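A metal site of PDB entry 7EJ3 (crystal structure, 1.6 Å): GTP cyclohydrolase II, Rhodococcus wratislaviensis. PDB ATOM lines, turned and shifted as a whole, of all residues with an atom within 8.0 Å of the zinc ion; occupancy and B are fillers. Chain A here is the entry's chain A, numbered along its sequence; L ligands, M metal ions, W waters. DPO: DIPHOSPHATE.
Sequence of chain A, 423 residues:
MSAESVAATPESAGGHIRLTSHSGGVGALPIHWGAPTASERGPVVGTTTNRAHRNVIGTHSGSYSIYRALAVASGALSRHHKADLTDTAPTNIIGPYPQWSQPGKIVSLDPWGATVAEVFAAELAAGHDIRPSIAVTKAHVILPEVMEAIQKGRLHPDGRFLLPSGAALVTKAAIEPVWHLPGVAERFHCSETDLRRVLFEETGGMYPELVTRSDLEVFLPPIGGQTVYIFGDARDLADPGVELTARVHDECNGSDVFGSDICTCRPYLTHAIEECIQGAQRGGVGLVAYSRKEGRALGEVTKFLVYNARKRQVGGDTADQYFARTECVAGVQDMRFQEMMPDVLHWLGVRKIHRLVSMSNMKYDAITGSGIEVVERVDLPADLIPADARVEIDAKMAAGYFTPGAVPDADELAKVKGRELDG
An oxygen (O3) of the ligand is in salt-bridge range of the side-chain amino group of Lys 396 (2.8 Å).
N of Ser 255 sits close to SG of Cys 252, at 3.7 Å.
The backbone NH of Arg 266 is in hydrogen-bond range of the side-chain hydroxyl of Ser 255.
OD2 of Asp 256 sits at hydrogen-bond distance from N of Cys 252 (2.9 Å).
The side-chain sulfur (SG) of Cys 252 lies close to the side-chain amino group (NZ) of Lys 303 (3.2 Å).
CB of Ser 255 touches the zinc ion, at 3.9 Å.
Within 4 Å of the zinc ion: Cys 252, Ser 255, Cys 263 and Cys 265.
The nearest printed residue that does not touch the zinc ion is Lys 303 (4.2 Å).
The zinc ion is bound by water W1 (2.2 Å), SG of Cys 265 (2.3 Å), SG of Cys 263 (2.3 Å) and SG of Cys 252 (2.3 Å).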
ATOM      1  N   HIS A 249     -37.170   9.903  19.872  1.00  0.00           N
ATOM      2  CA  HIS A 249     -36.055   8.995  20.100  1.00  0.00           C
ATOM      3  C   HIS A 249     -36.256   7.746  19.267  1.00  0.00           C
ATOM      4  O   HIS A 249     -37.315   7.103  19.361  1.00  0.00           O
ATOM      5  CB  HIS A 249     -35.986   8.638  21.581  1.00  0.00           C
ATOM      6  CG  HIS A 249     -34.743   7.925  21.976  1.00  0.00           C
ATOM      7  ND1 HIS A 249     -33.581   8.598  22.313  1.00  0.00           N
ATOM      8  CD2 HIS A 249     -34.460   6.607  22.098  1.00  0.00           C
ATOM      9  CE1 HIS A 249     -32.646   7.726  22.625  1.00  0.00           C
ATOM     10  NE2 HIS A 249     -33.155   6.504  22.505  1.00  0.00           N
ATOM     11  N   ASP A 250     -35.255   7.371  18.465  1.00  0.00           N
ATOM     12  CA  ASP A 250     -35.336   6.138  17.704  1.00  0.00           C
ATOM     13  C   ASP A 250     -34.662   4.992  18.459  1.00  0.00           C
ATOM     14  O   ASP A 250     -33.558   5.161  19.009  1.00  0.00           O
ATOM     15  CB  ASP A 250     -34.725   6.325  16.320  1.00  0.00           C
ATOM     16  CG  ASP A 250     -35.566   7.256  15.436  1.00  0.00           C
ATOM     17  OD1 ASP A 250     -36.810   7.089  15.419  1.00  0.00           O
ATOM     18  OD2 ASP A 250     -35.015   8.158  14.787  1.00  0.00           O
ATOM     19  N   GLU A 251     -35.326   3.838  18.501  1.00  0.00           N
ATOM     20  CA  GLU A 251     -34.886   2.704  19.321  1.00  0.00           C
ATOM     21  C   GLU A 251     -33.420   2.351  19.097  1.00  0.00           C
ATOM     22  O   GLU A 251     -32.955   2.226  17.968  1.00  0.00           O
ATOM     23  CB  GLU A 251     -35.747   1.486  19.004  1.00  0.00           C
ATOM     24  CG  GLU A 251     -35.325   0.248  19.775  1.00  0.00           C
ATOM     25  CD  GLU A 251     -36.226  -0.943  19.540  1.00  0.00           C
ATOM     26  OE1 GLU A 251     -37.099  -0.864  18.646  1.00  0.00           O
ATOM     27  OE2 GLU A 251     -36.046  -1.960  20.249  1.00  0.00           O
ATOM     28  N   CYS A 252     -32.717   2.138  20.222  1.00  0.00           N
ATOM     29  CA  CYS A 252     -31.373   1.555  20.264  1.00  0.00           C
ATOM     30  C   CYS A 252     -31.359   0.597  21.456  1.00  0.00           C
ATOM     31  O   CYS A 252     -31.109   1.009  22.590  1.00  0.00           O
ATOM     32  CB  CYS A 252     -30.310   2.624  20.428  1.00  0.00           C
ATOM     33  SG  CYS A 252     -28.644   1.929  20.620  1.00  0.00           S
ATOM     34  N   ASN A 253     -31.608  -0.693  21.210  1.00  0.00           N
ATOM     35  CA  ASN A 253     -31.737  -1.611  22.347  1.00  0.00           C
ATOM     36  C   ASN A 253     -30.442  -1.675  23.150  1.00  0.00           C
ATOM     37  O   ASN A 253     -30.474  -1.703  24.394  1.00  0.00           O
ATOM     38  CB  ASN A 253     -32.138  -3.002  21.876  1.00  0.00           C
ATOM     39  CG  ASN A 253     -32.436  -3.934  23.032  1.00  0.00           C
ATOM     40  OD1 ASN A 253     -31.627  -4.794  23.371  1.00  0.00           O
ATOM     41  ND2 ASN A 253     -33.578  -3.728  23.683  1.00  0.00           N
ATOM     42  N   GLY A 254     -29.303  -1.724  22.463  1.00  0.00           N
ATOM     43  CA  GLY A 254     -28.031  -1.928  23.127  1.00  0.00           C
ATOM     44  C   GLY A 254     -27.624  -0.802  24.055  1.00  0.00           C
ATOM     45  O   GLY A 254     -26.736  -0.988  24.886  1.00  0.00           O
ATOM     46  N   SER A 255     -28.239   0.377  23.905  1.00  0.00           N
ATOM     47  CA  SER A 255     -28.035   1.473  24.834  1.00  0.00           C
ATOM     48  C   SER A 255     -29.269   1.734  25.682  1.00  0.00           C
ATOM     49  O   SER A 255     -29.189   1.737  26.917  1.00  0.00           O
ATOM     50  CB  SER A 255     -27.652   2.748  24.070  1.00  0.00           C
ATOM     51  OG  SER A 255     -27.617   3.864  24.949  1.00  0.00           O
ATOM     52  N   ASP A 256     -30.431   1.907  25.035  1.00  0.00           N
ATOM     53  CA  ASP A 256     -31.670   2.210  25.741  1.00  0.00           C
ATOM     54  C   ASP A 256     -31.929   1.228  26.863  1.00  0.00           C
ATOM     55  O   ASP A 256     -32.445   1.603  27.921  1.00  0.00           O
ATOM     56  CB  ASP A 256     -32.849   2.193  24.766  1.00  0.00           C
ATOM     57  CG  ASP A 256     -32.770   3.264  23.690  1.00  0.00           C
ATOM     58  OD1 ASP A 256     -31.913   4.172  23.789  1.00  0.00           O
ATOM     59  OD2 ASP A 256     -33.584   3.198  22.767  1.00  0.00           O
ATOM     60  N   SER A 260     -24.706   0.297  26.412  1.00  0.00           N
ATOM     61  CA  SER A 260     -23.405   0.248  25.754  1.00  0.00           C
ATOM     62  C   SER A 260     -22.816   1.652  25.604  1.00  0.00           C
ATOM     63  O   SER A 260     -23.507   2.590  25.212  1.00  0.00           O
ATOM     64  CB  SER A 260     -23.531  -0.385  24.368  1.00  0.00           C
ATOM     65  OG  SER A 260     -22.334  -0.179  23.631  1.00  0.00           O
ATOM     66  N   ILE A 262     -20.802   2.841  23.436  1.00  0.00           N
ATOM     67  CA  ILE A 262     -20.407   3.248  22.094  1.00  0.00           C
ATOM     68  C   ILE A 262     -21.297   4.336  21.501  1.00  0.00           C
ATOM     69  O   ILE A 262     -20.943   4.878  20.442  1.00  0.00           O
ATOM     70  CB  ILE A 262     -20.395   2.056  21.112  1.00  0.00           C
ATOM     71  CG1 ILE A 262     -19.415   2.333  19.966  1.00  0.00           C
ATOM     72  CG2 ILE A 262     -21.817   1.770  20.593  1.00  0.00           C
ATOM     73  CD1 ILE A 262     -19.109   1.122  19.119  1.00  0.00           C
ATOM     74  N   CYS A 263     -22.410   4.678  22.143  1.00  0.00           N
ATOM     75  CA  CYS A 263     -23.337   5.638  21.529  1.00  0.00           C
ATOM     76  C   CYS A 263     -23.997   6.492  22.605  1.00  0.00           C
ATOM     77  O   CYS A 263     -23.872   6.252  23.808  1.00  0.00           O
ATOM     78  CB  CYS A 263     -24.395   4.918  20.672  1.00  0.00           C
ATOM     79  SG  CYS A 263     -25.458   3.782  21.609  1.00  0.00           S
ATOM     80  N   THR A 264     -24.708   7.509  22.139  1.00  0.00           N
ATOM     81  CA  THR A 264     -25.282   8.551  22.992  1.00  0.00           C
ATOM     82  C   THR A 264     -26.731   8.302  23.366  1.00  0.00           C
ATOM     83  O   THR A 264     -27.333   9.159  24.014  1.00  0.00           O
ATOM     84  CB  THR A 264     -25.184   9.905  22.289  1.00  0.00           C
ATOM     85  OG1 THR A 264     -25.811   9.811  21.006  1.00  0.00           O
ATOM     86  CG2 THR A 264     -23.743  10.363  22.099  1.00  0.00           C
ATOM     87  N   CYS A 265     -27.302   7.143  23.003  1.00  0.00           N
ATOM     88  CA  CYS A 265     -28.766   7.036  22.921  1.00  0.00           C
ATOM     89  C   CYS A 265     -29.442   7.145  24.281  1.00  0.00           C
ATOM     90  O   CYS A 265     -30.239   8.063  24.516  1.00  0.00           O
ATOM     91  CB  CYS A 265     -29.135   5.736  22.214  1.00  0.00           C
ATOM     92  SG  CYS A 265     -28.525   5.771  20.489  1.00  0.00           S
ATOM     93  N   ARG A 266     -29.180   6.210  25.194  1.00  0.00           N
ATOM     94  CA  ARG A 266     -29.855   6.299  26.492  1.00  0.00           C
ATOM     95  C   ARG A 266     -29.517   7.594  27.220  1.00  0.00           C
ATOM     96  O   ARG A 266     -30.430   8.193  27.820  1.00  0.00           O
ATOM     97  CB  ARG A 266     -29.543   5.080  27.375  1.00  0.00           C
ATOM     98  CG  ARG A 266     -30.441   5.068  28.628  1.00  0.00           C
ATOM     99  CD  ARG A 266     -30.348   3.824  29.509  1.00  0.00           C
ATOM    100  NE  ARG A 266     -30.958   4.069  30.802  1.00  0.00           N
ATOM    101  CZ  ARG A 266     -32.179   3.673  31.157  1.00  0.00           C
ATOM    102  NH1 ARG A 266     -32.928   2.941  30.351  1.00  0.00           N
ATOM    103  NH2 ARG A 266     -32.663   4.026  32.352  1.00  0.00           N
ATOM    104  N   PRO A 267     -28.287   8.078  27.214  1.00  0.00           N
ATOM    105  CA  PRO A 267     -28.046   9.407  27.810  1.00  0.00           C
ATOM    106  C   PRO A 267     -28.946  10.497  27.238  1.00  0.00           C
ATOM    107  O   PRO A 267     -29.459  11.313  28.014  1.00  0.00           O
ATOM    108  CB  PRO A 267     -26.563   9.658  27.482  1.00  0.00           C
ATOM    109  CG  PRO A 267     -25.971   8.266  27.469  1.00  0.00           C
ATOM    110  CD  PRO A 267     -27.036   7.408  26.811  1.00  0.00           C
ATOM    111  N   GLU A 294     -34.731   0.376  15.071  1.00  0.00           N
ATOM    112  CA  GLU A 294     -33.419  -0.077  15.517  1.00  0.00           C
ATOM    113  C   GLU A 294     -32.357   0.035  14.427  1.00  0.00           C
ATOM    114  O   GLU A 294     -32.562  -0.397  13.287  1.00  0.00           O
ATOM    115  CB  GLU A 294     -33.522  -1.536  15.995  1.00  0.00           C
ATOM    116  CG  GLU A 294     -32.185  -2.179  16.352  1.00  0.00           C
ATOM    117  CD  GLU A 294     -31.584  -1.633  17.645  1.00  0.00           C
ATOM    118  OE1 GLU A 294     -32.291  -1.627  18.677  1.00  0.00           O
ATOM    119  OE2 GLU A 294     -30.396  -1.208  17.626  1.00  0.00           O
ATOM    120  N   GLY A 295     -31.203   0.580  14.802  1.00  0.00           N
ATOM    121  CA  GLY A 295     -30.061   0.601  13.897  1.00  0.00           C
ATOM    122  C   GLY A 295     -30.289   1.447  12.662  1.00  0.00           C
ATOM    123  O   GLY A 295     -29.928   1.021  11.555  1.00  0.00           O
ATOM    124  N   LYS A 303     -26.248  -3.311  12.199  1.00  0.00           N
ATOM    125  CA  LYS A 303     -25.603  -2.412  13.142  1.00  0.00           C
ATOM    126  C   LYS A 303     -24.334  -3.032  13.729  1.00  0.00           C
ATOM    127  O   LYS A 303     -23.289  -2.372  13.811  1.00  0.00           O
ATOM    128  CB  LYS A 303     -26.604  -2.066  14.243  1.00  0.00           C
ATOM    129  CG  LYS A 303     -26.130  -1.120  15.332  1.00  0.00           C
ATOM    130  CD  LYS A 303     -27.316  -0.898  16.269  1.00  0.00           C
ATOM    131  CE  LYS A 303     -27.080   0.235  17.249  1.00  0.00           C
ATOM    132  NZ  LYS A 303     -28.413   0.721  17.720  1.00  0.00           N
ATOM    133  N   TYR A 307     -20.228  -2.095  13.435  1.00  0.00           N
ATOM    134  CA  TYR A 307     -19.332  -1.902  14.576  1.00  0.00           C
ATOM    135  C   TYR A 307     -18.027  -2.670  14.373  1.00  0.00           C
ATOM    136  O   TYR A 307     -16.940  -2.148  14.623  1.00  0.00           O
ATOM    137  CB  TYR A 307     -20.005  -2.372  15.871  1.00  0.00           C
ATOM    138  CG  TYR A 307     -21.086  -1.467  16.421  1.00  0.00           C
ATOM    139  CD1 TYR A 307     -21.154  -0.122  16.064  1.00  0.00           C
ATOM    140  CD2 TYR A 307     -22.025  -1.958  17.309  1.00  0.00           C
ATOM    141  CE1 TYR A 307     -22.145   0.699  16.588  1.00  0.00           C
ATOM    142  CE2 TYR A 307     -23.013  -1.161  17.838  1.00  0.00           C
ATOM    143  CZ  TYR A 307     -23.066   0.168  17.475  1.00  0.00           C
ATOM    144  OH  TYR A 307     -24.072   0.951  18.012  1.00  0.00           O
ATOM    145  N   TYR A 322     -16.836   7.046   9.936  1.00  0.00           N
ATOM    146  CA  TYR A 322     -18.014   6.504  10.619  1.00  0.00           C
ATOM    147  C   TYR A 322     -19.154   6.222   9.636  1.00  0.00           C
ATOM    148  O   TYR A 322     -19.736   5.128   9.650  1.00  0.00           O
ATOM    149  CB  TYR A 322     -18.438   7.512  11.700  1.00  0.00           C
ATOM    150  CG  TYR A 322     -19.785   7.286  12.386  1.00  0.00           C
ATOM    151  CD1 TYR A 322     -19.897   6.423  13.469  1.00  0.00           C
ATOM    152  CD2 TYR A 322     -20.926   7.988  11.987  1.00  0.00           C
ATOM    153  CE1 TYR A 322     -21.102   6.232  14.125  1.00  0.00           C
ATOM    154  CE2 TYR A 322     -22.141   7.799  12.632  1.00  0.00           C
ATOM    155  CZ  TYR A 322     -22.234   6.921  13.696  1.00  0.00           C
ATOM    156  OH  TYR A 322     -23.434   6.744  14.348  1.00  0.00           O
ATOM    157  N   GLU A 392     -19.073   8.702  17.174  1.00  0.00           N
ATOM    158  CA  GLU A 392     -20.453   8.924  16.720  1.00  0.00           C
ATOM    159  C   GLU A 392     -20.836  10.397  16.750  1.00  0.00           C
ATOM    160  O   GLU A 392     -21.300  10.958  15.742  1.00  0.00           O
ATOM    161  CB  GLU A 392     -21.410   8.108  17.592  1.00  0.00           C
ATOM    162  CG  GLU A 392     -22.887   8.483  17.387  1.00  0.00           C
ATOM    163  CD  GLU A 392     -23.631   8.653  18.700  1.00  0.00           C
ATOM    164  OE1 GLU A 392     -24.630   9.398  18.745  1.00  0.00           O
ATOM    165  OE2 GLU A 392     -23.235   8.012  19.701  1.00  0.00           O
ATOM    166  N   LYS A 396     -21.530  13.019  13.623  1.00  0.00           N
ATOM    167  CA  LYS A 396     -22.858  13.599  13.444  1.00  0.00           C
ATOM    168  C   LYS A 396     -22.797  15.121  13.392  1.00  0.00           C
ATOM    169  O   LYS A 396     -23.450  15.753  12.559  1.00  0.00           O
ATOM    170  CB  LYS A 396     -23.791  13.152  14.570  1.00  0.00           C
ATOM    171  CG  LYS A 396     -24.243  11.706  14.447  1.00  0.00           C
ATOM    172  CD  LYS A 396     -25.084  11.261  15.642  1.00  0.00           C
ATOM    173  CE  LYS A 396     -25.627   9.864  15.413  1.00  0.00           C
ATOM    174  NZ  LYS A 396     -26.360   9.351  16.605  1.00  0.00           N
HETATM  175  P1  DPO L   1     -30.241  10.634  16.071  1.00  0.00           P
HETATM  176  O1  DPO L   1     -31.408   9.754  16.448  1.00  0.00           O
HETATM  177  O2  DPO L   1     -29.996  10.597  14.578  1.00  0.00           O
HETATM  178  O3  DPO L   1     -28.971  10.307  16.820  1.00  0.00           O
HETATM  179  O4  DPO L   1     -30.673  12.182  16.387  1.00  0.00           O
HETATM  180  P2  DPO L   1     -30.712  12.942  17.837  1.00  0.00           P
HETATM  181  O5  DPO L   1     -32.158  13.286  18.101  1.00  0.00           O
HETATM  182  O6  DPO L   1     -29.867  14.195  17.711  1.00  0.00           O
HETATM  183  O7  DPO L   1     -30.211  12.029  18.914  1.00  0.00           O
HETATM  184 ZN    ZN M   1     -27.357   3.814  20.337  1.00  0.00          ZN
HETATM  185  O   HOH W   1     -26.803   3.936  18.233  1.00  0.00           O
